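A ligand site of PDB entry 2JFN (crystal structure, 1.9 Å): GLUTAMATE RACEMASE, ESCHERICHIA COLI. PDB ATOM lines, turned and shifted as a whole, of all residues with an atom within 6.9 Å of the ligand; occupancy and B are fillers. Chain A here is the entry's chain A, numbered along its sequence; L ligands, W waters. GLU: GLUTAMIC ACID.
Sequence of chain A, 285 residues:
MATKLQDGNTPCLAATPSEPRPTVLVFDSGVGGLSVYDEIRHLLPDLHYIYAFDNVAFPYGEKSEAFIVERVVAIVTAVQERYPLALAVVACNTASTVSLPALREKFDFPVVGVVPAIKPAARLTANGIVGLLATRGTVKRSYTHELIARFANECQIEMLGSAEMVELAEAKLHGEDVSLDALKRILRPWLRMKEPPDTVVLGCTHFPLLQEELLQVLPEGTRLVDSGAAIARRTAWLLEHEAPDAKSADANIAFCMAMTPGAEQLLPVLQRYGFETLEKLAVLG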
ATOM      1  N   ASP A  28       0.288 -16.956 -27.224  1.00  0.00           N
ATOM      2  CA  ASP A  28       0.327 -15.985 -26.127  1.00  0.00           C
ATOM      3  C   ASP A  28      -0.611 -16.470 -25.048  1.00  0.00           C
ATOM      4  O   ASP A  28      -1.431 -17.359 -25.269  1.00  0.00           O
ATOM      5  CB  ASP A  28      -0.140 -14.588 -26.573  1.00  0.00           C
ATOM      6  CG  ASP A  28      -0.016 -13.560 -25.439  1.00  0.00           C
ATOM      7  OD1 ASP A  28      -0.896 -12.682 -25.307  1.00  0.00           O
ATOM      8  OD2 ASP A  28       0.962 -13.645 -24.673  1.00  0.00           O
ATOM      9  N   SER A  29      -0.482 -15.883 -23.863  1.00  0.00           N
ATOM     10  CA  SER A  29      -1.344 -16.218 -22.735  1.00  0.00           C
ATOM     11  C   SER A  29      -2.735 -15.634 -22.991  1.00  0.00           C
ATOM     12  O   SER A  29      -3.747 -16.156 -22.525  1.00  0.00           O
ATOM     13  CB  SER A  29      -0.756 -15.644 -21.454  1.00  0.00           C
ATOM     14  OG  SER A  29      -0.625 -14.241 -21.572  1.00  0.00           O
ATOM     15  N   GLY A  30      -2.790 -14.534 -23.753  1.00  0.00           N
ATOM     16  CA  GLY A  30      -4.061 -13.909 -24.057  1.00  0.00           C
ATOM     17  C   GLY A  30      -4.145 -13.266 -25.435  1.00  0.00           C
ATOM     18  O   GLY A  30      -3.808 -13.902 -26.435  1.00  0.00           O
ATOM     19  N   VAL A  31      -4.569 -12.011 -25.483  1.00  0.00           N
ATOM     20  CA  VAL A  31      -4.709 -11.312 -26.756  1.00  0.00           C
ATOM     21  C   VAL A  31      -3.443 -10.597 -27.249  1.00  0.00           C
ATOM     22  O   VAL A  31      -3.362 -10.222 -28.419  1.00  0.00           O
ATOM     23  CB  VAL A  31      -5.864 -10.247 -26.705  1.00  0.00           C
ATOM     24  CG1 VAL A  31      -7.199 -10.940 -26.415  1.00  0.00           C
ATOM     25  CG2 VAL A  31      -5.583  -9.194 -25.634  1.00  0.00           C
ATOM     26  N   GLY A  32      -2.454 -10.421 -26.379  1.00  0.00           N
ATOM     27  CA  GLY A  32      -1.236  -9.734 -26.783  1.00  0.00           C
ATOM     28  C   GLY A  32      -0.579 -10.308 -28.027  1.00  0.00           C
ATOM     29  O   GLY A  32      -0.009  -9.589 -28.839  1.00  0.00           O
ATOM     30  N   GLY A  33      -0.668 -11.637 -28.181  1.00  0.00           N
ATOM     31  CA  GLY A  33      -0.082 -12.293 -29.331  1.00  0.00           C
ATOM     32  C   GLY A  33      -0.577 -11.722 -30.638  1.00  0.00           C
ATOM     33  O   GLY A  33       0.138 -11.734 -31.636  1.00  0.00           O
ATOM     34  N   ALA A  57      -4.804 -20.532 -18.072  1.00  0.00           N
ATOM     35  CA  ALA A  57      -3.763 -20.171 -17.120  1.00  0.00           C
ATOM     36  C   ALA A  57      -3.367 -18.693 -17.139  1.00  0.00           C
ATOM     37  O   ALA A  57      -2.500 -18.285 -16.367  1.00  0.00           O
ATOM     38  CB  ALA A  57      -2.551 -21.061 -17.322  1.00  0.00           C
ATOM     39  N   PHE A  58      -3.986 -17.905 -18.013  1.00  0.00           N
ATOM     40  CA  PHE A  58      -3.690 -16.468 -18.059  1.00  0.00           C
ATOM     41  C   PHE A  58      -4.121 -15.922 -16.694  1.00  0.00           C
ATOM     42  O   PHE A  58      -5.166 -16.325 -16.178  1.00  0.00           O
ATOM     43  CB  PHE A  58      -4.529 -15.795 -19.146  1.00  0.00           C
ATOM     44  CG  PHE A  58      -4.442 -14.292 -19.117  1.00  0.00           C
ATOM     45  CD1 PHE A  58      -3.435 -13.618 -19.802  1.00  0.00           C
ATOM     46  CD2 PHE A  58      -5.355 -13.546 -18.365  1.00  0.00           C
ATOM     47  CE1 PHE A  58      -3.315 -12.237 -19.730  1.00  0.00           C
ATOM     48  CE2 PHE A  58      -5.238 -12.152 -18.289  1.00  0.00           C
ATOM     49  CZ  PHE A  58      -4.218 -11.498 -18.972  1.00  0.00           C
ATOM     50  N   PRO A  59      -3.344 -15.005 -16.099  1.00  0.00           N
ATOM     51  CA  PRO A  59      -2.082 -14.405 -16.577  1.00  0.00           C
ATOM     52  C   PRO A  59      -0.837 -15.186 -16.177  1.00  0.00           C
ATOM     53  O   PRO A  59      -0.766 -15.768 -15.093  1.00  0.00           O
ATOM     54  CB  PRO A  59      -2.112 -13.013 -15.942  1.00  0.00           C
ATOM     55  CG  PRO A  59      -2.697 -13.309 -14.605  1.00  0.00           C
ATOM     56  CD  PRO A  59      -3.836 -14.273 -14.919  1.00  0.00           C
ATOM     57  N   TYR A  60       0.146 -15.200 -17.075  1.00  0.00           N
ATOM     58  CA  TYR A  60       1.417 -15.893 -16.844  1.00  0.00           C
ATOM     59  C   TYR A  60       2.352 -15.078 -15.924  1.00  0.00           C
ATOM     60  O   TYR A  60       3.193 -15.646 -15.225  1.00  0.00           O
ATOM     61  CB  TYR A  60       2.113 -16.154 -18.182  1.00  0.00           C
ATOM     62  CG  TYR A  60       1.623 -17.362 -18.965  1.00  0.00           C
ATOM     63  CD1 TYR A  60       0.397 -17.986 -18.660  1.00  0.00           C
ATOM     64  CD2 TYR A  60       2.380 -17.883 -20.017  1.00  0.00           C
ATOM     65  CE1 TYR A  60      -0.047 -19.104 -19.399  1.00  0.00           C
ATOM     66  CE2 TYR A  60       1.942 -18.987 -20.750  1.00  0.00           C
ATOM     67  CZ  TYR A  60       0.732 -19.585 -20.440  1.00  0.00           C
ATOM     68  OH  TYR A  60       0.315 -20.680 -21.181  1.00  0.00           O
ATOM     69  N   GLY A  61       2.188 -13.753 -15.931  1.00  0.00           N
ATOM     70  CA  GLY A  61       3.024 -12.891 -15.109  1.00  0.00           C
ATOM     71  C   GLY A  61       3.214 -13.333 -13.673  1.00  0.00           C
ATOM     72  O   GLY A  61       4.295 -13.196 -13.109  1.00  0.00           O
ATOM     73  N   GLU A  62       2.150 -13.863 -13.072  1.00  0.00           N
ATOM     74  CA  GLU A  62       2.176 -14.316 -11.683  1.00  0.00           C
ATOM     75  C   GLU A  62       2.702 -15.744 -11.500  1.00  0.00           C
ATOM     76  O   GLU A  62       3.370 -16.048 -10.497  1.00  0.00           O
ATOM     77  CB  GLU A  62       0.752 -14.247 -11.124  1.00  0.00           C
ATOM     78  CG  GLU A  62      -0.245 -15.019 -11.992  1.00  0.00           C
ATOM     79  CD  GLU A  62      -1.594 -15.183 -11.350  1.00  0.00           C
ATOM     80  OE1 GLU A  62      -2.264 -14.149 -11.082  1.00  0.00           O
ATOM     81  OE2 GLU A  62      -2.007 -16.348 -11.110  1.00  0.00           O
ATOM     82  N   ALA A  91       4.793 -15.311 -28.878  1.00  0.00           N
ATOM     83  CA  ALA A  91       4.564 -13.867 -28.834  1.00  0.00           C
ATOM     84  C   ALA A  91       4.074 -13.482 -27.451  1.00  0.00           C
ATOM     85  O   ALA A  91       2.992 -12.905 -27.295  1.00  0.00           O
ATOM     86  CB  ALA A  91       3.538 -13.478 -29.889  1.00  0.00           C
ATOM     87  N   CYS A  92       4.903 -13.792 -26.461  1.00  0.00           N
ATOM     88  CA  CYS A  92       4.595 -13.565 -25.062  1.00  0.00           C
ATOM     89  C   CYS A  92       5.915 -13.406 -24.295  1.00  0.00           C
ATOM     90  O   CYS A  92       6.690 -14.351 -24.203  1.00  0.00           O
ATOM     91  CB  CYS A  92       3.826 -14.795 -24.555  1.00  0.00           C
ATOM     92  SG  CYS A  92       3.513 -14.900 -22.804  1.00  0.00           S
ATOM     93  N   ASN A  93       6.162 -12.212 -23.744  1.00  0.00           N
ATOM     94  CA  ASN A  93       7.398 -11.958 -23.000  1.00  0.00           C
ATOM     95  C   ASN A  93       7.549 -12.810 -21.747  1.00  0.00           C
ATOM     96  O   ASN A  93       8.635 -13.319 -21.452  1.00  0.00           O
ATOM     97  CB  ASN A  93       7.494 -10.481 -22.602  1.00  0.00           C
ATOM     98  CG  ASN A  93       7.641  -9.562 -23.801  1.00  0.00           C
ATOM     99  OD1 ASN A  93       6.659  -9.266 -24.492  1.00  0.00           O
ATOM    100  ND2 ASN A  93       8.865  -9.112 -24.052  1.00  0.00           N
ATOM    101  N   THR A  94       6.466 -12.972 -20.997  1.00  0.00           N
ATOM    102  CA  THR A  94       6.500 -13.767 -19.773  1.00  0.00           C
ATOM    103  C   THR A  94       6.716 -15.256 -20.029  1.00  0.00           C
ATOM    104  O   THR A  94       6.897 -16.021 -19.091  1.00  0.00           O
ATOM    105  CB  THR A  94       5.195 -13.602 -18.955  1.00  0.00           C
ATOM    106  OG1 THR A  94       4.055 -13.860 -19.792  1.00  0.00           O
ATOM    107  CG2 THR A  94       5.087 -12.187 -18.401  1.00  0.00           C
ATOM    108  N   ALA A  95       6.699 -15.663 -21.292  1.00  0.00           N
ATOM    109  CA  ALA A  95       6.896 -17.073 -21.613  1.00  0.00           C
ATOM    110  C   ALA A  95       8.146 -17.325 -22.444  1.00  0.00           C
ATOM    111  O   ALA A  95       8.831 -18.325 -22.242  1.00  0.00           O
ATOM    112  CB  ALA A  95       5.667 -17.635 -22.331  1.00  0.00           C
ATOM    113  N   SER A  96       8.436 -16.411 -23.365  1.00  0.00           N
ATOM    114  CA  SER A  96       9.578 -16.573 -24.248  1.00  0.00           C
ATOM    115  C   SER A  96      10.852 -17.039 -23.558  1.00  0.00           C
ATOM    116  O   SER A  96      11.235 -18.204 -23.666  1.00  0.00           O
ATOM    117  CB  SER A  96       9.874 -15.282 -25.005  1.00  0.00           C
ATOM    118  OG  SER A  96       9.136 -15.234 -26.214  1.00  0.00           O
ATOM    119  N   VAL A 114      10.485 -13.657 -27.947  1.00  0.00           N
ATOM    120  CA  VAL A 114      10.376 -12.200 -27.846  1.00  0.00           C
ATOM    121  C   VAL A 114      11.014 -11.653 -26.582  1.00  0.00           C
ATOM    122  O   VAL A 114      10.824 -12.192 -25.488  1.00  0.00           O
ATOM    123  CB  VAL A 114       8.910 -11.746 -27.828  1.00  0.00           C
ATOM    124  CG1 VAL A 114       8.192 -12.208 -29.088  1.00  0.00           C
ATOM    125  CG2 VAL A 114       8.237 -12.262 -26.569  1.00  0.00           C
ATOM    126  N   THR A 135       4.820  -6.126 -17.971  1.00  0.00           N
ATOM    127  CA  THR A 135       3.903  -6.561 -16.930  1.00  0.00           C
ATOM    128  C   THR A 135       4.713  -6.701 -15.645  1.00  0.00           C
ATOM    129  O   THR A 135       5.950  -6.751 -15.667  1.00  0.00           O
ATOM    130  CB  THR A 135       3.209  -7.888 -17.303  1.00  0.00           C
ATOM    131  OG1 THR A 135       2.186  -8.146 -16.341  1.00  0.00           O
ATOM    132  CG2 THR A 135       4.207  -9.033 -17.335  1.00  0.00           C
ATOM    133  N   GLY A 137       5.439  -9.111 -13.621  1.00  0.00           N
ATOM    134  CA  GLY A 137       6.392 -10.201 -13.555  1.00  0.00           C
ATOM    135  C   GLY A 137       7.634 -10.054 -14.430  1.00  0.00           C
ATOM    136  O   GLY A 137       8.698 -10.573 -14.081  1.00  0.00           O
ATOM    137  N   THR A 138       7.503  -9.374 -15.554  1.00  0.00           N
ATOM    138  CA  THR A 138       8.622  -9.180 -16.478  1.00  0.00           C
ATOM    139  C   THR A 138       9.707  -8.228 -15.970  1.00  0.00           C
ATOM    140  O   THR A 138      10.874  -8.365 -16.331  1.00  0.00           O
ATOM    141  CB  THR A 138       8.120  -8.669 -17.841  1.00  0.00           C
ATOM    142  OG1 THR A 138       7.179  -9.608 -18.388  1.00  0.00           O
ATOM    143  CG2 THR A 138       9.279  -8.509 -18.817  1.00  0.00           C
ATOM    144  N   ALA A 163       0.517  -4.998 -14.305  1.00  0.00           N
ATOM    145  CA  ALA A 163      -0.363  -6.106 -14.631  1.00  0.00           C
ATOM    146  C   ALA A 163      -1.718  -5.522 -15.035  1.00  0.00           C
ATOM    147  O   ALA A 163      -2.456  -6.098 -15.827  1.00  0.00           O
ATOM    148  CB  ALA A 163      -0.520  -7.027 -13.435  1.00  0.00           C
ATOM    149  N   VAL A 166      -2.130  -4.853 -18.690  1.00  0.00           N
ATOM    150  CA  VAL A 166      -2.397  -6.066 -19.445  1.00  0.00           C
ATOM    151  C   VAL A 166      -3.909  -6.270 -19.477  1.00  0.00           C
ATOM    152  O   VAL A 166      -4.474  -6.597 -20.519  1.00  0.00           O
ATOM    153  CB  VAL A 166      -1.738  -7.299 -18.793  1.00  0.00           C
ATOM    154  CG1 VAL A 166      -2.090  -8.559 -19.588  1.00  0.00           C
ATOM    155  CG2 VAL A 166      -0.227  -7.109 -18.742  1.00  0.00           C
ATOM    156  N   GLU A 170      -6.683  -6.560 -22.463  1.00  0.00           N
ATOM    157  CA  GLU A 170      -7.650  -7.659 -22.570  1.00  0.00           C
ATOM    158  C   GLU A 170      -9.050  -7.073 -22.703  1.00  0.00           C
ATOM    159  O   GLU A 170      -9.800  -7.426 -23.611  1.00  0.00           O
ATOM    160  CB  GLU A 170      -7.579  -8.566 -21.329  1.00  0.00           C
ATOM    161  CG  GLU A 170      -6.392  -9.522 -21.293  1.00  0.00           C
ATOM    162  CD  GLU A 170      -6.528 -10.681 -22.280  1.00  0.00           C
ATOM    163  OE1 GLU A 170      -5.483 -11.133 -22.802  1.00  0.00           O
ATOM    164  OE2 GLU A 170      -7.658 -11.139 -22.533  1.00  0.00           O
ATOM    165  N   GLY A 203       7.419  -3.735 -23.639  1.00  0.00           N
ATOM    166  CA  GLY A 203       7.975  -5.051 -23.361  1.00  0.00           C
ATOM    167  C   GLY A 203       6.936  -6.092 -22.957  1.00  0.00           C
ATOM    168  O   GLY A 203       7.230  -7.033 -22.222  1.00  0.00           O
ATOM    169  N   CYS A 204       5.713  -5.878 -23.414  1.00  0.00           N
ATOM    170  CA  CYS A 204       4.617  -6.805 -23.160  1.00  0.00           C
ATOM    171  C   CYS A 204       3.857  -6.787 -24.477  1.00  0.00           C
ATOM    172  O   CYS A 204       3.468  -5.721 -24.955  1.00  0.00           O
ATOM    173  CB  CYS A 204       3.745  -6.310 -22.007  1.00  0.00           C
ATOM    174  SG  CYS A 204       2.506  -7.498 -21.488  1.00  0.00           S
ATOM    175  N   THR A 205       3.651  -7.950 -25.085  1.00  0.00           N
ATOM    176  CA  THR A 205       2.947  -7.991 -26.369  1.00  0.00           C
ATOM    177  C   THR A 205       1.510  -7.477 -26.299  1.00  0.00           C
ATOM    178  O   THR A 205       0.870  -7.237 -27.323  1.00  0.00           O
ATOM    179  CB  THR A 205       2.968  -9.412 -26.994  1.00  0.00           C
ATOM    180  OG1 THR A 205       2.210 -10.315 -26.172  1.00  0.00           O
ATOM    181  CG2 THR A 205       4.410  -9.924 -27.086  1.00  0.00           C
ATOM    182  N   HIS A 206       0.988  -7.310 -25.092  1.00  0.00           N
ATOM    183  CA  HIS A 206      -0.361  -6.777 -24.923  1.00  0.00           C
ATOM    184  C   HIS A 206      -0.371  -5.258 -25.150  1.00  0.00           C
ATOM    185  O   HIS A 206      -1.356  -4.691 -25.643  1.00  0.00           O
ATOM    186  CB  HIS A 206      -0.891  -7.023 -23.510  1.00  0.00           C
ATOM    187  CG  HIS A 206      -1.631  -8.316 -23.330  1.00  0.00           C
ATOM    188  ND1 HIS A 206      -0.997  -9.533 -23.277  1.00  0.00           N
ATOM    189  CD2 HIS A 206      -2.953  -8.569 -23.165  1.00  0.00           C
ATOM    190  CE1 HIS A 206      -1.898 -10.482 -23.075  1.00  0.00           C
ATOM    191  NE2 HIS A 206      -3.083  -9.918 -23.003  1.00  0.00           N
ATOM    192  N   PHE A 207       0.722  -4.602 -24.803  1.00  0.00           N
ATOM    193  CA  PHE A 207       0.792  -3.143 -24.886  1.00  0.00           C
ATOM    194  C   PHE A 207       0.646  -2.471 -26.241  1.00  0.00           C
ATOM    195  O   PHE A 207      -0.013  -1.427 -26.328  1.00  0.00           O
ATOM    196  CB  PHE A 207       2.045  -2.649 -24.130  1.00  0.00           C
ATOM    197  CG  PHE A 207       2.057  -3.020 -22.658  1.00  0.00           C
ATOM    198  CD1 PHE A 207       3.185  -2.800 -21.876  1.00  0.00           C
ATOM    199  CD2 PHE A 207       0.934  -3.614 -22.069  1.00  0.00           C
ATOM    200  CE1 PHE A 207       3.205  -3.162 -20.530  1.00  0.00           C
ATOM    201  CE2 PHE A 207       0.942  -3.984 -20.713  1.00  0.00           C
ATOM    202  CZ  PHE A 207       2.083  -3.757 -19.942  1.00  0.00           C
HETATM  203  N   GLU L   1       1.324 -11.012 -23.690  1.00  0.00           N
HETATM  204  CA  GLU L   1       1.905 -10.813 -22.357  1.00  0.00           C
HETATM  205  C   GLU L   1       3.414 -10.944 -22.449  1.00  0.00           C
HETATM  206  O   GLU L   1       4.022 -10.484 -23.487  1.00  0.00           O
HETATM  207  CB  GLU L   1       1.335 -11.865 -21.384  1.00  0.00           C
HETATM  208  CG  GLU L   1       0.924 -11.202 -20.055  1.00  0.00           C
HETATM  209  CD  GLU L   1       0.642 -12.244 -18.982  1.00  0.00           C
HETATM  210  OE1 GLU L   1       0.885 -11.996 -17.803  1.00  0.00           O
HETATM  211  OE2 GLU L   1       0.162 -13.347 -19.283  1.00  0.00           O
HETATM  212  OXT GLU L   1       4.065 -11.487 -21.503  1.00  0.00           O
HETATM  213  O   HOH W   1       0.336  -9.897 -16.202  1.00  0.00           O
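The side-chain hydroxyl (OG) of Ser 29 sits at hydrogen-bond distance from an oxygen (OE2) of the ligand (2.6 Å).
An oxygen (O) of the ligand sits at hydrogen-bond distance from the backbone NH (N) of Thr 205 (3.0 Å).
A nitrogen (N) of the ligand sits at hydrogen-bond distance from the side-chain hydroxyl (OG1) of Thr 205 (2.7 Å).
An oxygen (O) of the ligand sits at hydrogen-bond distance from the backbone NH (N) of Asn 93 (2.8 Å).
O of the ligand lies close to OD1 of Asn 93.
ND1 of His 206 sits at hydrogen-bond distance from N of the ligand (2.8 Å).
OD2 of Asp 28 lies within salt-bridge range of N of the ligand (2.8 Å).
N of Thr 94 is in hydrogen-bond range of OXT of the ligand (2.9 Å).
An oxygen (OXT) of the ligand is in hydrogen-bond range of the side-chain hydroxyl (OG1) of Thr 94 (2.9 Å).
OE1 of the ligand lies within hydrogen-bond range of N of Gly 61, 2.9 Å away.
N of Tyr 60 sits at hydrogen-bond distance from OE2 of the ligand (2.9 Å).
SG of Cys 92 lies within hydrogen-bond range of OXT of the ligand (3.7 Å).
Residues that only touch the ligand: Cys 204, Phe 58 and Pro 59.
Hydrophobic or aromatic side chains that line the ligand: Phe 58, Pro 59, Tyr 60 and His 206.
Of the 30 residues printed, 12 come within 4 Å of the ligand.
Along chain A the residues within 4 Å of the ligand span positions 28 to 206.
The nearest printed residue that does not touch the ligand is Val 166 (4.04 Å).
The backbone carbonyl oxygen (O) of Ala 91 lies within hydrogen-bond range of the side-chain hydroxyl (OG1) of Thr 205 (2.9 Å).
A ring nitrogen (NE2) of His 206 lies within hydrogen-bond range of the side-chain carboxylate (OE1) of Glu 170 (2.7 Å).
The side-chain sulfur (SG) of Cys 92 sits close to the side-chain carboxylate (OD2) of Asp 28, at 3.4 Å.
The backbone NH of Gly 32 lies within hydrogen-bond range of the side-chain carboxylate of Asp 28 (2.9 Å).
The backbone NH of Gly 33 lies within hydrogen-bond range of the side-chain carboxylate of Asp 28, 3.1 Å away.
The side-chain carboxylate of Asp 28 sits at hydrogen-bond distance from the backbone NH of Gly 30 (3.1 Å).
OG1 of Thr 94 sits at hydrogen-bond distance from SG of Cys 92 (3.2 Å).
O of Cys 92 is in hydrogen-bond range of OG of Ser 96, 3.3 Å away.
Water W1 bridges the side-chain hydroxyl (OG1) of Thr 135 (2.6 Å) and an oxygen (OE1) of the ligand (2.7 Å).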
